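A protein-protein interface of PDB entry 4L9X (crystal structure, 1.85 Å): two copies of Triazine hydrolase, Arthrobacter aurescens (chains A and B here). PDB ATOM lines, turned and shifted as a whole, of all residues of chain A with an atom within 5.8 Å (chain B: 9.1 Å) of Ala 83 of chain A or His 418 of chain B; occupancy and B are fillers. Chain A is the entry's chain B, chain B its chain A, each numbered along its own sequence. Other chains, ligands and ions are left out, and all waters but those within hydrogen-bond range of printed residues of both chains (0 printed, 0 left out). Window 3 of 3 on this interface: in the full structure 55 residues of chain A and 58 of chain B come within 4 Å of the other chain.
The backbone carbonyl oxygen (O) of Val 415 of chain B lies within hydrogen-bond range of the guanidinium group (NH1) of Arg 85 of chain A (3.0 Å). O of Ala 83 of chain A is in hydrogen-bond range of NE2 of His 418 of chain B (2.9 Å). The backbone NH (N) of His 418 of chain B sits at hydrogen-bond distance from the backbone carbonyl oxygen (O) of Arg 85 of chain A, at 2.8 Å. The backbone carbonyl oxygen (O) of Gly 82 of chain A sits close to the backbone carbonyl oxygen (O) of Val 415 of chain B (3.5 Å). N of Asp 419 of chain B sits at hydrogen-bond distance from O of Ala 86 of chain A (3.0 Å). The backbone NH of Arg 85 of chain A is in hydrogen-bond range of the backbone carbonyl oxygen of Gly 416 of chain B (3.5 Å).
The guanidinium group (NH1) of Arg 374 of chain B lies within salt-bridge range of the side-chain carboxylate (OD2) of Asp 419 of chain B (2.9 Å). OD1 of Asp 419 of chain B lies within hydrogen-bond range of N of Ala 421 of chain B, at 2.9 Å. The backbone carbonyl oxygen of Gly 416 of chain B lies close to a ring nitrogen (NE2) of His 418 of chain B (3.4 Å). The side-chain hydroxyl of Thr 427 of chain B is in hydrogen-bond range of the backbone carbonyl oxygen of Gly 423 of chain B (2.7 Å). The backbone NH (N) of Ile 422 of chain B sits at hydrogen-bond distance from the side-chain carboxylate (OD1) of Asp 419 of chain B, at 3.2 Å. The guanidinium group of Arg 414 of chain B sits at hydrogen-bond distance from the backbone carbonyl oxygen of Gly 423 of chain B, 3.2 Å away.
Among the printed residues, pairs that only touch across the chains: Gly 82 of chain A with Gly 416 of chain B, Ala 86 of chain A with His 418 of chain B, Arg 85 of chain A with Val 417 of chain B, Ile 87 of chain A with His 418 of chain B, Ala 86 of chain A with Gly 423 of chain B, Ala 86 of chain A with Ile 422 of chain B, Pro 88 of chain A with Ile 422 of chain B, Pro 88 of chain A with Asp 419 of chain B, Ile 465 of chain A with Gly 416 of chain B and Ala 86 of chain A with Val 417 of chain B.
Printed residues of chain B within 4 Å of Ala 83 of chain A: His 418. Of chain A, only Ala 83 (2.9 Å), Arg 85 (2.8 Å), Ala 86 (3.6 Å) and Ile 87 (3.7 Å) come within 4 Å of His 418 of chain B. Of chain B, only Val 415 (3.5 Å) and Gly 416 (3.4 Å) come within 4 Å of Gly 82 of chain A. Of the printed residues of chain A, Ile 422 of chain B touches Ala 86 and Pro 88. Printed residues of chain A within 4 Å of Val 415 of chain B: Gly 82 (3.5 Å) and Arg 85 (3.0 Å). Of the printed residues of chain B, Ile 465 of chain A touches Gly 416 (3.9 Å). Of the printed residues of chain B, Pro 88 of chain A touches Asp 419 (3.9 Å) and Ile 422 (3.8 Å). Glu 81 of chain A touches none of the printed residues of chain B. The nearest residue of chain A that does not touch His 418 of chain B is Met 84 of chain A (4.2 Å). The nearest printed residue of chain B that does not touch Pro 88 of chain A is His 418 of chain B (4.6 Å).
Of the 15 printed residues of chain A, 7 touch a printed residue of chain B. Of the 17 printed residues of chain B, 7 touch a printed residue of chain A. Among the printed residues, 16 pairs touch across the chains. Among the printed residues, no Asp or Glu carboxylate lies within 4 Å of a Lys or Arg side-chain nitrogen of the other chain.
No position is printed for both chains. Of the 16 pairs that touch across the chains among the printed residues, none has its exchanged pair printed and touching as well.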
ATOM      1  N   LEU A  79     -42.205  -9.415  -8.693  1.00  0.00           N
ATOM      2  CA  LEU A  79     -41.352  -8.581  -7.863  1.00  0.00           C
ATOM      3  C   LEU A  79     -40.371  -9.370  -6.957  1.00  0.00           C
ATOM      4  O   LEU A  79     -39.238  -8.911  -6.714  1.00  0.00           O
ATOM      5  CB  LEU A  79     -42.189  -7.587  -7.045  1.00  0.00           C
ATOM      6  CG  LEU A  79     -42.974  -6.570  -7.880  1.00  0.00           C
ATOM      7  CD1 LEU A  79     -43.958  -5.759  -7.016  1.00  0.00           C
ATOM      8  CD2 LEU A  79     -42.026  -5.649  -8.663  1.00  0.00           C
ATOM      9  N   TYR A  80     -40.775 -10.545  -6.476  1.00  0.00           N
ATOM     10  CA  TYR A  80     -39.877 -11.349  -5.623  1.00  0.00           C
ATOM     11  C   TYR A  80     -38.569 -11.723  -6.330  1.00  0.00           C
ATOM     12  O   TYR A  80     -37.549 -11.972  -5.676  1.00  0.00           O
ATOM     13  CB  TYR A  80     -40.563 -12.618  -5.077  1.00  0.00           C
ATOM     14  CG  TYR A  80     -40.917 -13.594  -6.158  1.00  0.00           C
ATOM     15  CD1 TYR A  80     -42.085 -13.444  -6.890  1.00  0.00           C
ATOM     16  CD2 TYR A  80     -40.069 -14.653  -6.474  1.00  0.00           C
ATOM     17  CE1 TYR A  80     -42.407 -14.309  -7.903  1.00  0.00           C
ATOM     18  CE2 TYR A  80     -40.383 -15.521  -7.488  1.00  0.00           C
ATOM     19  CZ  TYR A  80     -41.557 -15.343  -8.198  1.00  0.00           C
ATOM     20  OH  TYR A  80     -41.879 -16.207  -9.216  1.00  0.00           O
ATOM     21  N   GLU A  81     -38.594 -11.762  -7.661  1.00  0.00           N
ATOM     22  CA  GLU A  81     -37.403 -12.136  -8.425  1.00  0.00           C
ATOM     23  C   GLU A  81     -36.364 -11.020  -8.518  1.00  0.00           C
ATOM     24  O   GLU A  81     -35.280 -11.224  -9.070  1.00  0.00           O
ATOM     25  CB  GLU A  81     -37.778 -12.629  -9.831  1.00  0.00           C
ATOM     26  CG  GLU A  81     -38.547 -13.933  -9.835  1.00  0.00           C
ATOM     27  CD  GLU A  81     -39.019 -14.349 -11.216  1.00  0.00           C
ATOM     28  OE1 GLU A  81     -38.538 -13.779 -12.225  1.00  0.00           O
ATOM     29  OE2 GLU A  81     -39.877 -15.256 -11.289  1.00  0.00           O
ATOM     30  N   GLY A  82     -36.683  -9.836  -8.000  1.00  0.00           N
ATOM     31  CA  GLY A  82     -35.685  -8.785  -7.922  1.00  0.00           C
ATOM     32  C   GLY A  82     -34.489  -9.272  -7.110  1.00  0.00           C
ATOM     33  O   GLY A  82     -33.358  -8.794  -7.274  1.00  0.00           O
ATOM     34  N   ALA A  83     -34.741 -10.248  -6.247  1.00  0.00           N
ATOM     35  CA  ALA A  83     -33.709 -10.807  -5.375  1.00  0.00           C
ATOM     36  C   ALA A  83     -32.915 -11.910  -6.077  1.00  0.00           C
ATOM     37  O   ALA A  83     -31.963 -12.458  -5.510  1.00  0.00           O
ATOM     38  CB  ALA A  83     -34.355 -11.339  -4.094  1.00  0.00           C
ATOM     39  N   MET A  84     -33.300 -12.213  -7.317  1.00  0.00           N
ATOM     40  CA  MET A  84     -32.749 -13.355  -8.047  1.00  0.00           C
ATOM     41  C   MET A  84     -32.050 -12.967  -9.344  1.00  0.00           C
ATOM     42  O   MET A  84     -32.054 -13.736 -10.320  1.00  0.00           O
ATOM     43  CB  MET A  84     -33.855 -14.376  -8.334  1.00  0.00           C
ATOM     44  CG  MET A  84     -34.508 -14.921  -7.058  1.00  0.00           C
ATOM     45  SD  MET A  84     -35.838 -16.084  -7.393  1.00  0.00           S
ATOM     46  CE  MET A  84     -35.009 -17.223  -8.472  1.00  0.00           C
ATOM     47  N   ARG A  85     -31.433 -11.788  -9.346  1.00  0.00           N
ATOM     48  CA  ARG A  85     -30.791 -11.260 -10.546  1.00  0.00           C
ATOM     49  C   ARG A  85     -29.376 -11.769 -10.804  1.00  0.00           C
ATOM     50  O   ARG A  85     -28.566 -11.887  -9.882  1.00  0.00           O
ATOM     51  CB  ARG A  85     -30.755  -9.724 -10.508  1.00  0.00           C
ATOM     52  CG  ARG A  85     -32.087  -9.077 -10.833  1.00  0.00           C
ATOM     53  CD  ARG A  85     -32.065  -7.571 -10.577  1.00  0.00           C
ATOM     54  NE  ARG A  85     -33.249  -6.940 -11.154  1.00  0.00           N
ATOM     55  CZ  ARG A  85     -33.738  -5.761 -10.780  1.00  0.00           C
ATOM     56  NH1 ARG A  85     -33.145  -5.071  -9.823  1.00  0.00           N
ATOM     57  NH2 ARG A  85     -34.827  -5.275 -11.374  1.00  0.00           N
ATOM     58  N   ALA A  86     -29.085 -12.033 -12.079  1.00  0.00           N
ATOM     59  CA  ALA A  86     -27.711 -12.246 -12.532  1.00  0.00           C
ATOM     60  C   ALA A  86     -27.035 -13.345 -11.721  1.00  0.00           C
ATOM     61  O   ALA A  86     -25.871 -13.213 -11.333  1.00  0.00           O
ATOM     62  CB  ALA A  86     -26.901 -10.942 -12.444  1.00  0.00           C
ATOM     63  N   ILE A  87     -27.780 -14.412 -11.463  1.00  0.00           N
ATOM     64  CA  ILE A  87     -27.243 -15.594 -10.791  1.00  0.00           C
ATOM     65  C   ILE A  87     -26.533 -16.457 -11.836  1.00  0.00           C
ATOM     66  O   ILE A  87     -27.149 -16.871 -12.814  1.00  0.00           O
ATOM     67  CB  ILE A  87     -28.380 -16.405 -10.145  1.00  0.00           C
ATOM     68  CG1 ILE A  87     -29.013 -15.599  -9.005  1.00  0.00           C
ATOM     69  CG2 ILE A  87     -27.851 -17.753  -9.614  1.00  0.00           C
ATOM     70  CD1 ILE A  87     -30.320 -16.155  -8.505  1.00  0.00           C
ATOM     71  N   PRO A  88     -25.228 -16.714 -11.646  1.00  0.00           N
ATOM     72  CA  PRO A  88     -24.460 -17.452 -12.665  1.00  0.00           C
ATOM     73  C   PRO A  88     -25.107 -18.773 -13.091  1.00  0.00           C
ATOM     74  O   PRO A  88     -25.116 -19.074 -14.275  1.00  0.00           O
ATOM     75  CB  PRO A  88     -23.122 -17.710 -11.967  1.00  0.00           C
ATOM     76  CG  PRO A  88     -22.977 -16.548 -11.030  1.00  0.00           C
ATOM     77  CD  PRO A  88     -24.367 -16.235 -10.545  1.00  0.00           C
ATOM     78  N   TRP A 109     -35.478 -20.155   0.381  1.00  0.00           N
ATOM     79  CA  TRP A 109     -35.335 -18.898   1.099  1.00  0.00           C
ATOM     80  C   TRP A 109     -36.489 -18.707   2.071  1.00  0.00           C
ATOM     81  O   TRP A 109     -36.293 -18.316   3.217  1.00  0.00           O
ATOM     82  CB  TRP A 109     -35.285 -17.727   0.118  1.00  0.00           C
ATOM     83  CG  TRP A 109     -33.970 -17.573  -0.580  1.00  0.00           C
ATOM     84  CD1 TRP A 109     -32.771 -18.154  -0.237  1.00  0.00           C
ATOM     85  CD2 TRP A 109     -33.716 -16.785  -1.748  1.00  0.00           C
ATOM     86  NE1 TRP A 109     -31.786 -17.772  -1.128  1.00  0.00           N
ATOM     87  CE2 TRP A 109     -32.341 -16.932  -2.064  1.00  0.00           C
ATOM     88  CE3 TRP A 109     -34.518 -15.973  -2.563  1.00  0.00           C
ATOM     89  CZ2 TRP A 109     -31.756 -16.294  -3.163  1.00  0.00           C
ATOM     90  CZ3 TRP A 109     -33.938 -15.341  -3.644  1.00  0.00           C
ATOM     91  CH2 TRP A 109     -32.565 -15.497  -3.935  1.00  0.00           C
ATOM     92  N   PHE A 115     -37.113 -14.895   3.621  1.00  0.00           N
ATOM     93  CA  PHE A 115     -37.936 -14.321   2.570  1.00  0.00           C
ATOM     94  C   PHE A 115     -39.288 -13.898   3.117  1.00  0.00           C
ATOM     95  O   PHE A 115     -40.306 -14.074   2.458  1.00  0.00           O
ATOM     96  CB  PHE A 115     -38.116 -15.344   1.448  1.00  0.00           C
ATOM     97  CG  PHE A 115     -37.955 -14.769   0.065  1.00  0.00           C
ATOM     98  CD1 PHE A 115     -37.144 -13.666  -0.152  1.00  0.00           C
ATOM     99  CD2 PHE A 115     -38.623 -15.331  -1.014  1.00  0.00           C
ATOM    100  CE1 PHE A 115     -37.009 -13.122  -1.428  1.00  0.00           C
ATOM    101  CE2 PHE A 115     -38.491 -14.796  -2.294  1.00  0.00           C
ATOM    102  CZ  PHE A 115     -37.679 -13.692  -2.497  1.00  0.00           C
ATOM    103  N   VAL A 123     -37.823  -5.568  -1.415  1.00  0.00           N
ATOM    104  CA  VAL A 123     -37.472  -5.954  -2.779  1.00  0.00           C
ATOM    105  C   VAL A 123     -38.473  -5.292  -3.724  1.00  0.00           C
ATOM    106  O   VAL A 123     -38.093  -4.711  -4.740  1.00  0.00           O
ATOM    107  CB  VAL A 123     -37.541  -7.484  -2.963  1.00  0.00           C
ATOM    108  CG1 VAL A 123     -37.490  -7.855  -4.445  1.00  0.00           C
ATOM    109  CG2 VAL A 123     -36.417  -8.171  -2.183  1.00  0.00           C
ATOM    110  N   ILE A 465     -31.547  -8.750   0.938  1.00  0.00           N
ATOM    111  CA  ILE A 465     -31.474  -9.798  -0.077  1.00  0.00           C
ATOM    112  C   ILE A 465     -30.923 -11.056   0.596  1.00  0.00           C
ATOM    113  O   ILE A 465     -29.953 -10.972   1.349  1.00  0.00           O
ATOM    114  CB  ILE A 465     -30.548  -9.403  -1.254  1.00  0.00           C
ATOM    115  CG1 ILE A 465     -31.023  -8.111  -1.932  1.00  0.00           C
ATOM    116  CG2 ILE A 465     -30.453 -10.532  -2.272  1.00  0.00           C
ATOM    117  CD1 ILE A 465     -32.278  -8.271  -2.754  1.00  0.00           C
ATOM    118  N   PRO A 466     -31.547 -12.221   0.347  1.00  0.00           N
ATOM    119  CA  PRO A 466     -31.070 -13.451   0.991  1.00  0.00           C
ATOM    120  C   PRO A 466     -29.615 -13.745   0.652  1.00  0.00           C
ATOM    121  O   PRO A 466     -29.222 -13.645  -0.513  1.00  0.00           O
ATOM    122  CB  PRO A 466     -31.989 -14.527   0.406  1.00  0.00           C
ATOM    123  CG  PRO A 466     -33.250 -13.796   0.086  1.00  0.00           C
ATOM    124  CD  PRO A 466     -32.794 -12.446  -0.412  1.00  0.00           C
ATOM    125  N   THR B  21     -15.033  -2.397  -6.427  1.00  0.00           N
ATOM    126  CA  THR B  21     -15.771  -3.571  -5.969  1.00  0.00           C
ATOM    127  C   THR B  21     -15.413  -4.832  -6.750  1.00  0.00           C
ATOM    128  O   THR B  21     -15.214  -5.904  -6.170  1.00  0.00           O
ATOM    129  CB  THR B  21     -17.296  -3.327  -6.005  1.00  0.00           C
ATOM    130  OG1 THR B  21     -17.639  -2.381  -4.985  1.00  0.00           O
ATOM    131  CG2 THR B  21     -18.066  -4.628  -5.759  1.00  0.00           C
ATOM    132  N   ARG B  22     -15.335  -4.706  -8.073  1.00  0.00           N
ATOM    133  CA  ARG B  22     -14.920  -5.826  -8.915  1.00  0.00           C
ATOM    134  C   ARG B  22     -14.051  -5.284 -10.041  1.00  0.00           C
ATOM    135  O   ARG B  22     -14.339  -4.218 -10.606  1.00  0.00           O
ATOM    136  CB  ARG B  22     -16.142  -6.568  -9.488  1.00  0.00           C
ATOM    137  CG  ARG B  22     -15.809  -7.740 -10.441  1.00  0.00           C
ATOM    138  CD  ARG B  22     -15.337  -8.991  -9.694  1.00  0.00           C
ATOM    139  NE  ARG B  22     -16.368  -9.501  -8.789  1.00  0.00           N
ATOM    140  CZ  ARG B  22     -17.101 -10.591  -9.012  1.00  0.00           C
ATOM    141  NH1 ARG B  22     -16.911 -11.331 -10.101  1.00  0.00           N
ATOM    142  NH2 ARG B  22     -18.020 -10.958  -8.125  1.00  0.00           N
ATOM    143  N   GLU B  34     -11.603  -8.506  -6.295  1.00  0.00           N
ATOM    144  CA  GLU B  34     -12.583  -7.790  -5.477  1.00  0.00           C
ATOM    145  C   GLU B  34     -11.888  -6.768  -4.576  1.00  0.00           C
ATOM    146  O   GLU B  34     -10.770  -7.001  -4.117  1.00  0.00           O
ATOM    147  CB  GLU B  34     -13.394  -8.761  -4.614  1.00  0.00           C
ATOM    148  CG  GLU B  34     -14.425  -9.577  -5.365  1.00  0.00           C
ATOM    149  CD  GLU B  34     -15.488 -10.160  -4.427  1.00  0.00           C
ATOM    150  OE1 GLU B  34     -15.221 -10.296  -3.202  1.00  0.00           O
ATOM    151  OE2 GLU B  34     -16.596 -10.476  -4.916  1.00  0.00           O
ATOM    152  N   ARG B 374     -19.658 -12.984 -19.986  1.00  0.00           N
ATOM    153  CA  ARG B 374     -18.217 -12.773 -19.983  1.00  0.00           C
ATOM    154  C   ARG B 374     -17.620 -12.902 -21.372  1.00  0.00           C
ATOM    155  O   ARG B 374     -16.661 -12.221 -21.690  1.00  0.00           O
ATOM    156  CB  ARG B 374     -17.516 -13.712 -18.993  1.00  0.00           C
ATOM    157  CG  ARG B 374     -17.686 -13.244 -17.546  1.00  0.00           C
ATOM    158  CD  ARG B 374     -17.120 -14.217 -16.515  1.00  0.00           C
ATOM    159  NE  ARG B 374     -17.067 -13.565 -15.206  1.00  0.00           N
ATOM    160  CZ  ARG B 374     -18.134 -13.352 -14.444  1.00  0.00           C
ATOM    161  NH1 ARG B 374     -19.334 -13.750 -14.857  1.00  0.00           N
ATOM    162  NH2 ARG B 374     -18.001 -12.743 -13.270  1.00  0.00           N
ATOM    163  N   LEU B 409     -22.397   0.015  -9.353  1.00  0.00           N
ATOM    164  CA  LEU B 409     -23.209  -1.170  -9.097  1.00  0.00           C
ATOM    165  C   LEU B 409     -24.291  -0.929  -8.055  1.00  0.00           C
ATOM    166  O   LEU B 409     -25.108  -1.809  -7.804  1.00  0.00           O
ATOM    167  CB  LEU B 409     -22.325  -2.306  -8.595  1.00  0.00           C
ATOM    168  CG  LEU B 409     -21.202  -2.760  -9.529  1.00  0.00           C
ATOM    169  CD1 LEU B 409     -20.206  -3.559  -8.729  1.00  0.00           C
ATOM    170  CD2 LEU B 409     -21.771  -3.586 -10.678  1.00  0.00           C
ATOM    171  N   ARG B 414     -30.089  -2.002  -9.896  1.00  0.00           N
ATOM    172  CA  ARG B 414     -29.174  -3.141  -9.858  1.00  0.00           C
ATOM    173  C   ARG B 414     -29.144  -3.823  -8.495  1.00  0.00           C
ATOM    174  O   ARG B 414     -28.242  -4.605  -8.202  1.00  0.00           O
ATOM    175  CB  ARG B 414     -27.758  -2.743 -10.309  1.00  0.00           C
ATOM    176  CG  ARG B 414     -27.694  -2.122 -11.705  1.00  0.00           C
ATOM    177  CD  ARG B 414     -26.260  -2.113 -12.183  1.00  0.00           C
ATOM    178  NE  ARG B 414     -25.989  -1.225 -13.312  1.00  0.00           N
ATOM    179  CZ  ARG B 414     -26.087  -1.561 -14.595  1.00  0.00           C
ATOM    180  NH1 ARG B 414     -26.489  -2.776 -14.956  1.00  0.00           N
ATOM    181  NH2 ARG B 414     -25.775  -0.672 -15.525  1.00  0.00           N
ATOM    182  N   VAL B 415     -30.151  -3.535  -7.675  1.00  0.00           N
ATOM    183  CA  VAL B 415     -30.342  -4.258  -6.421  1.00  0.00           C
ATOM    184  C   VAL B 415     -30.605  -5.736  -6.729  1.00  0.00           C
ATOM    185  O   VAL B 415     -31.272  -6.067  -7.722  1.00  0.00           O
ATOM    186  CB  VAL B 415     -31.531  -3.667  -5.641  1.00  0.00           C
ATOM    187  CG1 VAL B 415     -31.978  -4.613  -4.546  1.00  0.00           C
ATOM    188  CG2 VAL B 415     -31.166  -2.296  -5.072  1.00  0.00           C
ATOM    189  N   GLY B 416     -30.069  -6.630  -5.900  1.00  0.00           N
ATOM    190  CA  GLY B 416     -30.266  -8.054  -6.124  1.00  0.00           C
ATOM    191  C   GLY B 416     -29.324  -8.731  -7.107  1.00  0.00           C
ATOM    192  O   GLY B 416     -29.379  -9.946  -7.270  1.00  0.00           O
ATOM    193  N   VAL B 417     -28.481  -7.958  -7.791  1.00  0.00           N
ATOM    194  CA  VAL B 417     -27.550  -8.538  -8.759  1.00  0.00           C
ATOM    195  C   VAL B 417     -26.548  -9.435  -8.037  1.00  0.00           C
ATOM    196  O   VAL B 417     -25.899  -9.006  -7.086  1.00  0.00           O
ATOM    197  CB  VAL B 417     -26.782  -7.442  -9.506  1.00  0.00           C
ATOM    198  CG1 VAL B 417     -25.533  -8.006 -10.201  1.00  0.00           C
ATOM    199  CG2 VAL B 417     -27.706  -6.753 -10.517  1.00  0.00           C
ATOM    200  N   HIS B 418     -26.428 -10.678  -8.475  1.00  0.00           N
ATOM    201  CA  HIS B 418     -25.491 -11.591  -7.803  1.00  0.00           C
ATOM    202  C   HIS B 418     -24.093 -11.508  -8.401  1.00  0.00           C
ATOM    203  O   HIS B 418     -23.112 -11.333  -7.675  1.00  0.00           O
ATOM    204  CB  HIS B 418     -26.036 -13.015  -7.772  1.00  0.00           C
ATOM    205  CG  HIS B 418     -27.240 -13.159  -6.893  1.00  0.00           C
ATOM    206  ND1 HIS B 418     -27.284 -14.018  -5.812  1.00  0.00           N
ATOM    207  CD2 HIS B 418     -28.432 -12.511  -6.907  1.00  0.00           C
ATOM    208  CE1 HIS B 418     -28.461 -13.913  -5.214  1.00  0.00           C
ATOM    209  NE2 HIS B 418     -29.175 -13.003  -5.857  1.00  0.00           N
ATOM    210  N   ASP B 419     -24.009 -11.554  -9.728  1.00  0.00           N
ATOM    211  CA  ASP B 419     -22.728 -11.479 -10.421  1.00  0.00           C
ATOM    212  C   ASP B 419     -22.683 -10.175 -11.217  1.00  0.00           C
ATOM    213  O   ASP B 419     -23.487  -9.986 -12.118  1.00  0.00           O
ATOM    214  CB  ASP B 419     -22.592 -12.689 -11.351  1.00  0.00           C
ATOM    215  CG  ASP B 419     -21.324 -12.661 -12.171  1.00  0.00           C
ATOM    216  OD1 ASP B 419     -20.963 -11.606 -12.712  1.00  0.00           O
ATOM    217  OD2 ASP B 419     -20.683 -13.718 -12.289  1.00  0.00           O
ATOM    218  N   PRO B 420     -21.761  -9.262 -10.870  1.00  0.00           N
ATOM    219  CA  PRO B 420     -21.794  -7.927 -11.491  1.00  0.00           C
ATOM    220  C   PRO B 420     -21.457  -7.906 -12.984  1.00  0.00           C
ATOM    221  O   PRO B 420     -21.922  -7.003 -13.678  1.00  0.00           O
ATOM    222  CB  PRO B 420     -20.760  -7.132 -10.678  1.00  0.00           C
ATOM    223  CG  PRO B 420     -19.851  -8.188 -10.083  1.00  0.00           C
ATOM    224  CD  PRO B 420     -20.760  -9.347  -9.788  1.00  0.00           C
ATOM    225  N   ALA B 421     -20.677  -8.863 -13.489  1.00  0.00           N
ATOM    226  CA  ALA B 421     -20.424  -8.902 -14.926  1.00  0.00           C
ATOM    227  C   ALA B 421     -21.707  -9.242 -15.698  1.00  0.00           C
ATOM    228  O   ALA B 421     -22.042  -8.593 -16.696  1.00  0.00           O
ATOM    229  CB  ALA B 421     -19.309  -9.890 -15.258  1.00  0.00           C
ATOM    230  N   ILE B 422     -22.420 -10.261 -15.235  1.00  0.00           N
ATOM    231  CA  ILE B 422     -23.692 -10.629 -15.847  1.00  0.00           C
ATOM    232  C   ILE B 422     -24.656  -9.452 -15.641  1.00  0.00           C
ATOM    233  O   ILE B 422     -25.441  -9.113 -16.526  1.00  0.00           O
ATOM    234  CB  ILE B 422     -24.266 -11.906 -15.214  1.00  0.00           C
ATOM    235  CG1 ILE B 422     -23.296 -13.085 -15.432  1.00  0.00           C
ATOM    236  CG2 ILE B 422     -25.652 -12.215 -15.781  1.00  0.00           C
ATOM    237  CD1 ILE B 422     -23.768 -14.376 -14.803  1.00  0.00           C
ATOM    238  N   GLY B 423     -24.566  -8.830 -14.468  1.00  0.00           N
ATOM    239  CA  GLY B 423     -25.392  -7.671 -14.150  1.00  0.00           C
ATOM    240  C   GLY B 423     -25.284  -6.530 -15.154  1.00  0.00           C
ATOM    241  O   GLY B 423     -26.295  -5.935 -15.527  1.00  0.00           O
ATOM    242  N   LEU B 424     -24.062  -6.227 -15.597  1.00  0.00           N
ATOM    243  CA  LEU B 424     -23.817  -5.173 -16.593  1.00  0.00           C
ATOM    244  C   LEU B 424     -24.562  -5.411 -17.900  1.00  0.00           C
ATOM    245  O   LEU B 424     -24.997  -4.465 -18.572  1.00  0.00           O
ATOM    246  CB  LEU B 424     -22.317  -5.064 -16.921  1.00  0.00           C
ATOM    247  CG  LEU B 424     -21.480  -4.012 -16.211  1.00  0.00           C
ATOM    248  CD1 LEU B 424     -20.127  -3.899 -16.910  1.00  0.00           C
ATOM    249  CD2 LEU B 424     -22.175  -2.656 -16.195  1.00  0.00           C
ATOM    250  N   THR B 427     -29.100  -6.284 -16.671  1.00  0.00           N
ATOM    251  CA  THR B 427     -29.948  -5.383 -15.875  1.00  0.00           C
ATOM    252  C   THR B 427     -29.692  -3.919 -16.214  1.00  0.00           C
ATOM    253  O   THR B 427     -28.741  -3.590 -16.932  1.00  0.00           O
ATOM    254  CB  THR B 427     -29.671  -5.527 -14.364  1.00  0.00           C
ATOM    255  OG1 THR B 427     -28.349  -5.039 -14.087  1.00  0.00           O
ATOM    256  CG2 THR B 427     -29.784  -6.988 -13.923  1.00  0.00           C
